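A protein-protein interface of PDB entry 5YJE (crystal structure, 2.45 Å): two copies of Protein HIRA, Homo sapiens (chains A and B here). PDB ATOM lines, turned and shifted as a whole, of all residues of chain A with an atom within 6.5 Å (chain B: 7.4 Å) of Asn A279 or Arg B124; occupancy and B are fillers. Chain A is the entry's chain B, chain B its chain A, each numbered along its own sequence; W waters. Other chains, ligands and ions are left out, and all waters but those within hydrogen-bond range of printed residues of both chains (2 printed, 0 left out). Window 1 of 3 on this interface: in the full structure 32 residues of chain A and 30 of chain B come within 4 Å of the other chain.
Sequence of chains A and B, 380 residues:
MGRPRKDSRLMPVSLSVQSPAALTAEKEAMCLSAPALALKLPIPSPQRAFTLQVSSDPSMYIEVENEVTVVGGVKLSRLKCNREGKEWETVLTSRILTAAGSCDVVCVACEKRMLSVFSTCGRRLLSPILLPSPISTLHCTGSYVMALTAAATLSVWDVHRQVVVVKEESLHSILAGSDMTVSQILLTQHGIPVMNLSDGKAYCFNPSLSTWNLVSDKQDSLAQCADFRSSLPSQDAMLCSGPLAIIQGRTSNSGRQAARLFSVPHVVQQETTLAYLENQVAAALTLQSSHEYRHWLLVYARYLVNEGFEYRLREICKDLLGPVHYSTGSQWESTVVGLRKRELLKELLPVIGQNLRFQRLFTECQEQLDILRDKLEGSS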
ATOM      1  N   LEU A 214       9.980  31.147  19.568  1.00  0.00           N
ATOM      2  CA  LEU A 214       8.783  31.963  19.401  1.00  0.00           C
ATOM      3  C   LEU A 214       7.940  31.886  20.667  1.00  0.00           C
ATOM      4  O   LEU A 214       7.329  30.856  20.953  1.00  0.00           O
ATOM      5  CB  LEU A 214       7.985  31.478  18.196  1.00  0.00           C
ATOM      6  CG  LEU A 214       6.758  32.316  17.886  1.00  0.00           C
ATOM      7  CD1 LEU A 214       7.182  33.684  17.315  1.00  0.00           C
ATOM      8  CD2 LEU A 214       5.855  31.553  16.931  1.00  0.00           C
ATOM      9  N   VAL A 215       7.890  32.979  21.422  1.00  0.00           N
ATOM     10  CA  VAL A 215       7.165  33.025  22.685  1.00  0.00           C
ATOM     11  C   VAL A 215       5.917  33.874  22.595  1.00  0.00           C
ATOM     12  O   VAL A 215       5.204  34.014  23.593  1.00  0.00           O
ATOM     13  CB  VAL A 215       8.069  33.541  23.823  1.00  0.00           C
ATOM     14  CG1 VAL A 215       9.249  32.631  23.972  1.00  0.00           C
ATOM     15  CG2 VAL A 215       8.539  34.983  23.533  1.00  0.00           C
ATOM     16  N   LEU A 222      -3.922  32.215  19.516  1.00  0.00           N
ATOM     17  CA  LEU A 222      -5.118  31.480  19.888  1.00  0.00           C
ATOM     18  C   LEU A 222      -5.783  32.049  21.128  1.00  0.00           C
ATOM     19  O   LEU A 222      -6.771  31.477  21.604  1.00  0.00           O
ATOM     20  CB  LEU A 222      -4.776  30.009  20.105  1.00  0.00           C
ATOM     21  CG  LEU A 222      -4.289  29.287  18.859  1.00  0.00           C
ATOM     22  CD1 LEU A 222      -3.359  28.159  19.253  1.00  0.00           C
ATOM     23  CD2 LEU A 222      -5.477  28.758  18.068  1.00  0.00           C
ATOM     24  N   LEU A 244       6.743  37.892  29.921  1.00  0.00           N
ATOM     25  CA  LEU A 244       5.739  37.408  28.969  1.00  0.00           C
ATOM     26  C   LEU A 244       4.544  38.350  28.865  1.00  0.00           C
ATOM     27  O   LEU A 244       4.077  38.665  27.762  1.00  0.00           O
ATOM     28  CB  LEU A 244       5.248  36.006  29.362  1.00  0.00           C
ATOM     29  CG  LEU A 244       4.363  35.239  28.363  1.00  0.00           C
ATOM     30  CD1 LEU A 244       5.115  34.892  27.093  1.00  0.00           C
ATOM     31  CD2 LEU A 244       3.795  33.978  28.990  1.00  0.00           C
ATOM     32  N   GLN A 248       3.704  40.173  25.275  1.00  0.00           N
ATOM     33  CA  GLN A 248       2.363  40.140  24.732  1.00  0.00           C
ATOM     34  C   GLN A 248       1.628  41.428  25.092  1.00  0.00           C
ATOM     35  O   GLN A 248       2.054  42.200  25.950  1.00  0.00           O
ATOM     36  CB  GLN A 248       1.645  38.895  25.248  1.00  0.00           C
ATOM     37  CG  GLN A 248       2.452  37.644  24.955  1.00  0.00           C
ATOM     38  CD  GLN A 248       1.928  36.411  25.642  1.00  0.00           C
ATOM     39  OE1 GLN A 248       1.234  36.504  26.651  1.00  0.00           O
ATOM     40  NE2 GLN A 248       2.282  35.241  25.117  1.00  0.00           N
ATOM     41  N   LEU A 274      -6.286  24.322  24.865  1.00  0.00           N
ATOM     42  CA  LEU A 274      -5.155  23.540  25.346  1.00  0.00           C
ATOM     43  C   LEU A 274      -3.848  24.017  24.708  1.00  0.00           C
ATOM     44  O   LEU A 274      -2.851  24.244  25.403  1.00  0.00           O
ATOM     45  CB  LEU A 274      -5.381  22.065  25.037  1.00  0.00           C
ATOM     46  CG  LEU A 274      -5.730  21.020  26.100  1.00  0.00           C
ATOM     47  CD1 LEU A 274      -5.372  19.660  25.567  1.00  0.00           C
ATOM     48  CD2 LEU A 274      -5.033  21.236  27.403  1.00  0.00           C
ATOM     49  N   ALA A 275      -3.840  24.165  23.379  1.00  0.00           N
ATOM     50  CA  ALA A 275      -2.648  24.614  22.676  1.00  0.00           C
ATOM     51  C   ALA A 275      -2.201  25.979  23.179  1.00  0.00           C
ATOM     52  O   ALA A 275      -1.016  26.192  23.448  1.00  0.00           O
ATOM     53  CB  ALA A 275      -2.905  24.655  21.171  1.00  0.00           C
ATOM     54  N   TYR A 276      -3.150  26.897  23.359  1.00  0.00           N
ATOM     55  CA  TYR A 276      -2.834  28.216  23.880  1.00  0.00           C
ATOM     56  C   TYR A 276      -2.201  28.141  25.263  1.00  0.00           C
ATOM     57  O   TYR A 276      -1.167  28.777  25.513  1.00  0.00           O
ATOM     58  CB  TYR A 276      -4.086  29.082  23.929  1.00  0.00           C
ATOM     59  CG  TYR A 276      -3.853  30.391  24.674  1.00  0.00           C
ATOM     60  CD1 TYR A 276      -3.068  31.393  24.114  1.00  0.00           C
ATOM     61  CD2 TYR A 276      -4.392  30.613  25.945  1.00  0.00           C
ATOM     62  CE1 TYR A 276      -2.843  32.589  24.779  1.00  0.00           C
ATOM     63  CE2 TYR A 276      -4.185  31.814  26.615  1.00  0.00           C
ATOM     64  CZ  TYR A 276      -3.405  32.799  26.018  1.00  0.00           C
ATOM     65  OH  TYR A 276      -3.166  33.993  26.651  1.00  0.00           O
ATOM     66  N   LEU A 277      -2.830  27.415  26.191  1.00  0.00           N
ATOM     67  CA  LEU A 277      -2.318  27.402  27.559  1.00  0.00           C
ATOM     68  C   LEU A 277      -0.966  26.695  27.643  1.00  0.00           C
ATOM     69  O   LEU A 277      -0.094  27.097  28.426  1.00  0.00           O
ATOM     70  CB  LEU A 277      -3.339  26.769  28.509  1.00  0.00           C
ATOM     71  CG  LEU A 277      -4.618  27.579  28.798  1.00  0.00           C
ATOM     72  CD1 LEU A 277      -5.669  26.743  29.526  1.00  0.00           C
ATOM     73  CD2 LEU A 277      -4.322  28.850  29.599  1.00  0.00           C
ATOM     74  N   GLU A 278      -0.768  25.653  26.833  1.00  0.00           N
ATOM     75  CA  GLU A 278       0.539  25.010  26.755  1.00  0.00           C
ATOM     76  C   GLU A 278       1.588  25.966  26.182  1.00  0.00           C
ATOM     77  O   GLU A 278       2.729  25.988  26.639  1.00  0.00           O
ATOM     78  CB  GLU A 278       0.437  23.724  25.925  1.00  0.00           C
ATOM     79  CG  GLU A 278      -0.273  22.584  26.643  1.00  0.00           C
ATOM     80  CD  GLU A 278      -0.633  21.383  25.737  1.00  0.00           C
ATOM     81  OE1 GLU A 278      -1.303  20.455  26.239  1.00  0.00           O
ATOM     82  OE2 GLU A 278      -0.252  21.353  24.535  1.00  0.00           O
ATOM     83  N   ASN A 279       1.213  26.751  25.177  1.00  0.00           N
ATOM     84  CA  ASN A 279       2.083  27.788  24.639  1.00  0.00           C
ATOM     85  C   ASN A 279       2.486  28.787  25.718  1.00  0.00           C
ATOM     86  O   ASN A 279       3.656  29.156  25.819  1.00  0.00           O
ATOM     87  CB  ASN A 279       1.384  28.520  23.492  1.00  0.00           C
ATOM     88  CG  ASN A 279       1.471  27.770  22.167  1.00  0.00           C
ATOM     89  OD1 ASN A 279       2.398  26.991  21.942  1.00  0.00           O
ATOM     90  ND2 ASN A 279       0.503  28.014  21.274  1.00  0.00           N
ATOM     91  N   GLN A 280       1.525  29.237  26.530  1.00  0.00           N
ATOM     92  CA  GLN A 280       1.816  30.181  27.612  1.00  0.00           C
ATOM     93  C   GLN A 280       2.784  29.588  28.624  1.00  0.00           C
ATOM     94  O   GLN A 280       3.751  30.243  29.033  1.00  0.00           O
ATOM     95  CB  GLN A 280       0.521  30.596  28.320  1.00  0.00           C
ATOM     96  CG  GLN A 280      -0.404  31.465  27.503  1.00  0.00           C
ATOM     97  CD  GLN A 280       0.291  32.728  27.023  1.00  0.00           C
ATOM     98  OE1 GLN A 280       1.010  32.701  26.029  1.00  0.00           O
ATOM     99  NE2 GLN A 280       0.081  33.843  27.733  1.00  0.00           N
ATOM    100  N   VAL A 281       2.521  28.352  29.057  1.00  0.00           N
ATOM    101  CA  VAL A 281       3.388  27.689  30.030  1.00  0.00           C
ATOM    102  C   VAL A 281       4.804  27.559  29.466  1.00  0.00           C
ATOM    103  O   VAL A 281       5.794  27.935  30.110  1.00  0.00           O
ATOM    104  CB  VAL A 281       2.789  26.318  30.418  1.00  0.00           C
ATOM    105  CG1 VAL A 281       3.718  25.515  31.327  1.00  0.00           C
ATOM    106  CG2 VAL A 281       1.414  26.486  31.080  1.00  0.00           C
ATOM    107  N   ALA A 282       4.907  27.045  28.238  1.00  0.00           N
ATOM    108  CA  ALA A 282       6.197  26.874  27.597  1.00  0.00           C
ATOM    109  C   ALA A 282       6.909  28.215  27.423  1.00  0.00           C
ATOM    110  O   ALA A 282       8.125  28.310  27.593  1.00  0.00           O
ATOM    111  CB  ALA A 282       6.009  26.193  26.246  1.00  0.00           C
ATOM    112  N   ALA A 283       6.163  29.256  27.065  1.00  0.00           N
ATOM    113  CA  ALA A 283       6.763  30.553  26.839  1.00  0.00           C
ATOM    114  C   ALA A 283       7.324  31.094  28.138  1.00  0.00           C
ATOM    115  O   ALA A 283       8.420  31.670  28.162  1.00  0.00           O
ATOM    116  CB  ALA A 283       5.732  31.511  26.241  1.00  0.00           C
ATOM    117  N   ALA A 284       6.600  30.879  29.236  1.00  0.00           N
ATOM    118  CA  ALA A 284       7.080  31.362  30.522  1.00  0.00           C
ATOM    119  C   ALA A 284       8.332  30.604  30.953  1.00  0.00           C
ATOM    120  O   ALA A 284       9.278  31.210  31.464  1.00  0.00           O
ATOM    121  CB  ALA A 284       5.968  31.261  31.567  1.00  0.00           C
ATOM    122  N   TYR A 300      -3.316  26.185  33.670  1.00  0.00           N
ATOM    123  CA  TYR A 300      -3.340  25.037  32.776  1.00  0.00           C
ATOM    124  C   TYR A 300      -3.810  23.783  33.496  1.00  0.00           C
ATOM    125  O   TYR A 300      -4.589  22.992  32.947  1.00  0.00           O
ATOM    126  CB  TYR A 300      -1.948  24.832  32.182  1.00  0.00           C
ATOM    127  CG  TYR A 300      -1.797  23.602  31.323  1.00  0.00           C
ATOM    128  CD1 TYR A 300      -2.544  23.440  30.159  1.00  0.00           C
ATOM    129  CD2 TYR A 300      -0.887  22.612  31.659  1.00  0.00           C
ATOM    130  CE1 TYR A 300      -2.398  22.312  29.367  1.00  0.00           C
ATOM    131  CE2 TYR A 300      -0.739  21.483  30.875  1.00  0.00           C
ATOM    132  CZ  TYR A 300      -1.492  21.334  29.743  1.00  0.00           C
ATOM    133  OH  TYR A 300      -1.313  20.203  28.983  1.00  0.00           O
ATOM    134  N   ARG A 312      -2.792  13.978  30.221  1.00  0.00           N
ATOM    135  CA  ARG A 312      -1.964  15.173  30.324  1.00  0.00           C
ATOM    136  C   ARG A 312      -1.697  15.545  31.778  1.00  0.00           C
ATOM    137  O   ARG A 312      -0.555  15.867  32.142  1.00  0.00           O
ATOM    138  CB  ARG A 312      -2.624  16.337  29.571  1.00  0.00           C
ATOM    139  CG  ARG A 312      -2.401  16.338  28.059  1.00  0.00           C
ATOM    140  CD  ARG A 312      -3.231  17.421  27.391  1.00  0.00           C
ATOM    141  NE  ARG A 312      -2.996  17.494  25.953  1.00  0.00           N
ATOM    142  CZ  ARG A 312      -3.626  16.738  25.057  1.00  0.00           C
ATOM    143  NH1 ARG A 312      -3.357  16.866  23.764  1.00  0.00           N
ATOM    144  NH2 ARG A 312      -4.529  15.853  25.449  1.00  0.00           N
ATOM    145  N   THR B  90      -3.582  17.352  18.780  1.00  0.00           N
ATOM    146  CA  THR B  90      -3.419  18.754  19.089  1.00  0.00           C
ATOM    147  C   THR B  90      -3.469  19.546  17.796  1.00  0.00           C
ATOM    148  O   THR B  90      -3.528  18.990  16.693  1.00  0.00           O
ATOM    149  CB  THR B  90      -2.111  18.994  19.853  1.00  0.00           C
ATOM    150  OG1 THR B  90      -2.134  20.316  20.369  1.00  0.00           O
ATOM    151  CG2 THR B  90      -0.918  18.803  18.949  1.00  0.00           C
ATOM    152  N   VAL B  91      -3.450  20.860  17.953  1.00  0.00           N
ATOM    153  CA  VAL B  91      -3.503  21.769  16.820  1.00  0.00           C
ATOM    154  C   VAL B  91      -2.240  22.636  16.830  1.00  0.00           C
ATOM    155  O   VAL B  91      -1.665  22.916  17.885  1.00  0.00           O
ATOM    156  CB  VAL B  91      -4.798  22.619  16.858  1.00  0.00           C
ATOM    157  CG1 VAL B  91      -6.052  21.727  16.645  1.00  0.00           C
ATOM    158  CG2 VAL B  91      -4.914  23.377  18.178  1.00  0.00           C
ATOM    159  N   LEU B  92      -1.792  23.017  15.634  1.00  0.00           N
ATOM    160  CA  LEU B  92      -0.729  23.989  15.420  1.00  0.00           C
ATOM    161  C   LEU B  92      -1.255  25.097  14.511  1.00  0.00           C
ATOM    162  O   LEU B  92      -2.229  24.907  13.781  1.00  0.00           O
ATOM    163  CB  LEU B  92       0.526  23.319  14.817  1.00  0.00           C
ATOM    164  CG  LEU B  92       1.199  22.442  15.888  1.00  0.00           C
ATOM    165  CD1 LEU B  92       0.720  20.969  15.862  1.00  0.00           C
ATOM    166  CD2 LEU B  92       2.734  22.571  15.909  1.00  0.00           C
ATOM    167  N   THR B  93      -0.613  26.268  14.555  1.00  0.00           N
ATOM    168  CA  THR B  93      -1.109  27.402  13.785  1.00  0.00           C
ATOM    169  C   THR B  93      -0.379  27.581  12.463  1.00  0.00           C
ATOM    170  O   THR B  93      -0.476  28.644  11.845  1.00  0.00           O
ATOM    171  CB  THR B  93      -1.061  28.695  14.607  1.00  0.00           C
ATOM    172  OG1 THR B  93       0.294  29.029  14.915  1.00  0.00           O
ATOM    173  CG2 THR B  93      -1.849  28.529  15.893  1.00  0.00           C
ATOM    174  N   CYS B 110       7.306  22.547  10.934  1.00  0.00           N
ATOM    175  CA  CYS B 110       6.304  23.387  10.312  1.00  0.00           C
ATOM    176  C   CYS B 110       6.935  24.445   9.415  1.00  0.00           C
ATOM    177  O   CYS B 110       8.076  24.882   9.616  1.00  0.00           O
ATOM    178  CB  CYS B 110       5.441  24.083  11.370  1.00  0.00           C
ATOM    179  SG  CYS B 110       4.665  22.945  12.525  1.00  0.00           S
ATOM    180  N   LEU B 115       9.970  24.421  14.685  1.00  0.00           N
ATOM    181  CA  LEU B 115      10.113  23.074  15.218  1.00  0.00           C
ATOM    182  C   LEU B 115       9.349  23.001  16.529  1.00  0.00           C
ATOM    183  O   LEU B 115       9.651  23.759  17.454  1.00  0.00           O
ATOM    184  CB  LEU B 115      11.598  22.740  15.440  1.00  0.00           C
ATOM    185  CG  LEU B 115      11.996  21.290  15.712  1.00  0.00           C
ATOM    186  CD1 LEU B 115      13.478  21.084  15.488  1.00  0.00           C
ATOM    187  CD2 LEU B 115      11.625  20.875  17.117  1.00  0.00           C
ATOM    188  N   SER B 116       8.397  22.066  16.634  1.00  0.00           N
ATOM    189  CA  SER B 116       7.612  21.903  17.855  1.00  0.00           C
ATOM    190  C   SER B 116       7.747  20.492  18.420  1.00  0.00           C
ATOM    191  O   SER B 116       7.855  19.509  17.687  1.00  0.00           O
ATOM    192  CB  SER B 116       6.136  22.238  17.623  1.00  0.00           C
ATOM    193  OG  SER B 116       5.946  23.629  17.528  1.00  0.00           O
ATOM    194  N   VAL B 117       7.735  20.398  19.745  1.00  0.00           N
ATOM    195  CA  VAL B 117       8.018  19.147  20.438  1.00  0.00           C
ATOM    196  C   VAL B 117       6.931  18.900  21.478  1.00  0.00           C
ATOM    197  O   VAL B 117       6.621  19.777  22.291  1.00  0.00           O
ATOM    198  CB  VAL B 117       9.411  19.167  21.094  1.00  0.00           C
ATOM    199  CG1 VAL B 117       9.655  17.871  21.840  1.00  0.00           C
ATOM    200  CG2 VAL B 117      10.483  19.396  20.037  1.00  0.00           C
ATOM    201  N   PHE B 118       6.358  17.713  21.447  1.00  0.00           N
ATOM    202  CA  PHE B 118       5.219  17.345  22.270  1.00  0.00           C
ATOM    203  C   PHE B 118       5.558  16.074  23.026  1.00  0.00           C
ATOM    204  O   PHE B 118       6.389  15.272  22.588  1.00  0.00           O
ATOM    205  CB  PHE B 118       3.955  17.151  21.420  1.00  0.00           C
ATOM    206  CG  PHE B 118       3.587  18.358  20.619  1.00  0.00           C
ATOM    207  CD1 PHE B 118       4.127  18.559  19.357  1.00  0.00           C
ATOM    208  CD2 PHE B 118       2.713  19.303  21.133  1.00  0.00           C
ATOM    209  CE1 PHE B 118       3.799  19.693  18.607  1.00  0.00           C
ATOM    210  CE2 PHE B 118       2.377  20.444  20.396  1.00  0.00           C
ATOM    211  CZ  PHE B 118       2.920  20.639  19.128  1.00  0.00           C
ATOM    212  N   SER B 119       4.907  15.908  24.172  1.00  0.00           N
ATOM    213  CA  SER B 119       5.144  14.766  25.046  1.00  0.00           C
ATOM    214  C   SER B 119       4.571  13.484  24.444  1.00  0.00           C
ATOM    215  O   SER B 119       3.913  13.481  23.394  1.00  0.00           O
ATOM    216  CB  SER B 119       4.517  15.013  26.410  1.00  0.00           C
ATOM    217  OG  SER B 119       3.103  14.943  26.267  1.00  0.00           O
ATOM    218  N   CYS B 121       2.080  12.056  25.388  1.00  0.00           N
ATOM    219  CA  CYS B 121       0.630  12.222  25.354  1.00  0.00           C
ATOM    220  C   CYS B 121       0.204  13.592  24.815  1.00  0.00           C
ATOM    221  O   CYS B 121      -0.876  14.081  25.143  1.00  0.00           O
ATOM    222  CB  CYS B 121       0.032  11.977  26.740  1.00  0.00           C
ATOM    223  SG  CYS B 121       0.310  13.310  27.909  1.00  0.00           S
ATOM    224  N   GLY B 122       1.042  14.230  23.999  1.00  0.00           N
ATOM    225  CA  GLY B 122       0.615  15.364  23.194  1.00  0.00           C
ATOM    226  C   GLY B 122       0.667  16.734  23.830  1.00  0.00           C
ATOM    227  O   GLY B 122       0.146  17.689  23.236  1.00  0.00           O
ATOM    228  N   ARG B 123       1.257  16.868  25.011  1.00  0.00           N
ATOM    229  CA  ARG B 123       1.462  18.176  25.618  1.00  0.00           C
ATOM    230  C   ARG B 123       2.707  18.838  25.026  1.00  0.00           C
ATOM    231  O   ARG B 123       3.788  18.243  25.018  1.00  0.00           O
ATOM    232  CB  ARG B 123       1.595  18.004  27.127  1.00  0.00           C
ATOM    233  CG  ARG B 123       1.701  19.264  27.929  1.00  0.00           C
ATOM    234  CD  ARG B 123       1.851  18.876  29.389  1.00  0.00           C
ATOM    235  NE  ARG B 123       2.858  17.827  29.558  1.00  0.00           N
ATOM    236  CZ  ARG B 123       4.103  18.051  29.980  1.00  0.00           C
ATOM    237  NH1 ARG B 123       4.492  19.287  30.285  1.00  0.00           N
ATOM    238  NH2 ARG B 123       4.959  17.040  30.101  1.00  0.00           N
ATOM    239  N   ARG B 124       2.551  20.057  24.506  1.00  0.00           N
ATOM    240  CA  ARG B 124       3.699  20.833  24.042  1.00  0.00           C
ATOM    241  C   ARG B 124       4.743  20.946  25.147  1.00  0.00           C
ATOM    242  O   ARG B 124       4.438  21.361  26.267  1.00  0.00           O
ATOM    243  CB  ARG B 124       3.257  22.233  23.584  1.00  0.00           C
ATOM    244  CG  ARG B 124       4.442  23.161  23.323  1.00  0.00           C
ATOM    245  CD  ARG B 124       4.084  24.544  22.771  1.00  0.00           C
ATOM    246  NE  ARG B 124       3.485  24.471  21.443  1.00  0.00           N
ATOM    247  CZ  ARG B 124       4.166  24.371  20.307  1.00  0.00           C
ATOM    248  NH1 ARG B 124       5.501  24.343  20.322  1.00  0.00           N
ATOM    249  NH2 ARG B 124       3.511  24.318  19.151  1.00  0.00           N
ATOM    250  N   LEU B 125       5.976  20.564  24.832  1.00  0.00           N
ATOM    251  CA  LEU B 125       7.068  20.571  25.803  1.00  0.00           C
ATOM    252  C   LEU B 125       7.880  21.861  25.782  1.00  0.00           C
ATOM    253  O   LEU B 125       8.254  22.373  26.842  1.00  0.00           O
ATOM    254  CB  LEU B 125       7.990  19.371  25.556  1.00  0.00           C
ATOM    255  CG  LEU B 125       7.284  18.020  25.786  1.00  0.00           C
ATOM    256  CD1 LEU B 125       8.187  16.825  25.517  1.00  0.00           C
ATOM    257  CD2 LEU B 125       6.768  17.933  27.213  1.00  0.00           C
ATOM    258  N   LEU B 126       8.130  22.408  24.600  1.00  0.00           N
ATOM    259  CA  LEU B 126       8.963  23.589  24.424  1.00  0.00           C
ATOM    260  C   LEU B 126       8.253  24.570  23.506  1.00  0.00           C
ATOM    261  O   LEU B 126       7.488  24.164  22.623  1.00  0.00           O
ATOM    262  CB  LEU B 126      10.325  23.213  23.817  1.00  0.00           C
ATOM    263  CG  LEU B 126      11.035  22.043  24.509  1.00  0.00           C
ATOM    264  CD1 LEU B 126      12.156  21.452  23.682  1.00  0.00           C
ATOM    265  CD2 LEU B 126      11.528  22.501  25.857  1.00  0.00           C
ATOM    266  N   SER B 127       8.503  25.869  23.734  1.00  0.00           N
ATOM    267  CA  SER B 127       8.171  26.912  22.770  1.00  0.00           C
ATOM    268  C   SER B 127       8.701  26.520  21.401  1.00  0.00           C
ATOM    269  O   SER B 127       9.745  25.866  21.310  1.00  0.00           O
ATOM    270  CB  SER B 127       8.764  28.262  23.170  1.00  0.00           C
ATOM    271  OG  SER B 127       8.429  28.599  24.497  1.00  0.00           O
ATOM    272  N   PRO B 128       8.018  26.891  20.323  1.00  0.00           N
ATOM    273  CA  PRO B 128       8.526  26.575  18.982  1.00  0.00           C
ATOM    274  C   PRO B 128       9.944  27.096  18.809  1.00  0.00           C
ATOM    275  O   PRO B 128      10.295  28.181  19.285  1.00  0.00           O
ATOM    276  CB  PRO B 128       7.547  27.299  18.049  1.00  0.00           C
ATOM    277  CG  PRO B 128       6.306  27.505  18.866  1.00  0.00           C
ATOM    278  CD  PRO B 128       6.762  27.662  20.289  1.00  0.00           C
ATOM    279  N   ILE B 129      10.752  26.314  18.112  1.00  0.00           N
ATOM    280  CA  ILE B 129      12.162  26.601  17.898  1.00  0.00           C
ATOM    281  C   ILE B 129      12.321  27.106  16.471  1.00  0.00           C
ATOM    282  O   ILE B 129      11.936  26.425  15.515  1.00  0.00           O
ATOM    283  CB  ILE B 129      13.020  25.346  18.145  1.00  0.00           C
ATOM    284  CG1 ILE B 129      13.054  25.033  19.639  1.00  0.00           C
ATOM    285  CG2 ILE B 129      14.404  25.482  17.497  1.00  0.00           C
ATOM    286  CD1 ILE B 129      13.537  23.664  19.972  1.00  0.00           C
HETATM  287  O   HOH W   1       3.723  23.714  27.684  1.00  0.00           O
HETATM  288  O   HOH W   2      -0.623  21.999  22.116  1.00  0.00           O
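N of Arg B124 sits at hydrogen-bond distance from OE2 of Glu A278, at 3.1 Å.
The side-chain amide oxygen (OD1) of Asn A279 lies within hydrogen-bond range of the guanidinium group (NE) of Arg B124 (2.8 Å).
The backbone carbonyl oxygen (O) of Ala A282 lies within hydrogen-bond range of the side-chain hydroxyl (OG) of Ser B127 (3.1 Å).
OG of Ser B127 sits close to N of Ala A283.
The backbone NH (N) of Leu A214 lies within hydrogen-bond range of the backbone carbonyl oxygen (O) of Pro B128.
The side-chain hydroxyl (OG) of Ser B116 is in hydrogen-bond range of the guanidinium group (NH1) of Arg B124 (2.9 Å).
The side-chain hydroxyl (OG) of Ser B119 sits at hydrogen-bond distance from the backbone NH (N) of Gly B122 (3.1 Å).
The side-chain hydroxyl (OG) of Ser B119 is in hydrogen-bond range of the backbone NH (N) of Arg B123 (2.9 Å).
O of Ala A275 lies close to ND2 of Asn A279, at 3.2 Å.
OE1 of Glu A278 is in hydrogen-bond range of OH of Tyr A300 (2.8 Å).
OE1 of Glu A278 is in salt-bridge range of NE of Arg A312, 3.4 Å away.
Among the printed residues, merely in contact across the chains: Leu A214 with Ser B127, Leu A222 with Thr B93, Ala A275 with Val B91, Glu A278 with Gly B122, Glu A278 with Arg B123, Ala A282 with Leu B126, Tyr A300 with Arg B123, Arg A312 with Cys B121 and Arg A312 with Gly B122.
Printed residues of chain B within 4 Å of Glu A278: Gly B122, Arg B123 and Arg B124.
Of chain B, only Arg B124 comes within 4 Å of Asn A279.
Printed residues of chain B within 4 Å of Tyr A300: Arg B123.
Cys B110 touches none of the printed residues of chain A.
Of chain A, only Glu A278 (3.1 Å) and Asn A279 (2.8 Å) come within 4 Å of Arg B124.
Printed residues of chain A within 4 Å of Leu B126: Ala A282 (3.9 Å).
The nearest residue of chain B that does not touch Asn A279 is Pro B128 (4.7 Å).
The nearest residue of chain A that does not touch Arg B124 is Ala A282 (4.3 Å).
The nearest printed residue of chain A that does not touch Cys B121 is Glu A278 (6.5 Å).
Printed residues of chain B that touch a printed residue of chain A: Val B91, Thr B93, Cys B121, Gly B122, Arg B123, Arg B124, Leu B126, Ser B127 and Pro B128.
Printed residues of chain A that touch a printed residue of chain B: Leu A214, Leu A222, Ala A275, Glu A278, Asn A279, Ala A282, Ala A283, Tyr A300 and Arg A312.
Hydrophobic or aromatic side chains of chain A within 4 Å of the printed part of chain B: Leu A222, Ala A275, Ala A282 and Tyr A300.
No position is printed for both chains.
Water W2 bridges the side-chain carboxylate (OE2) of Glu A278 (2.5 Å) and the side-chain hydroxyl (OG1) of Thr B90 (2.9 Å).
Water W1 lies within hydrogen-bond range of the backbone carbonyl oxygen (O) of Glu A278 and the backbone carbonyl oxygen (O) of Arg B124.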
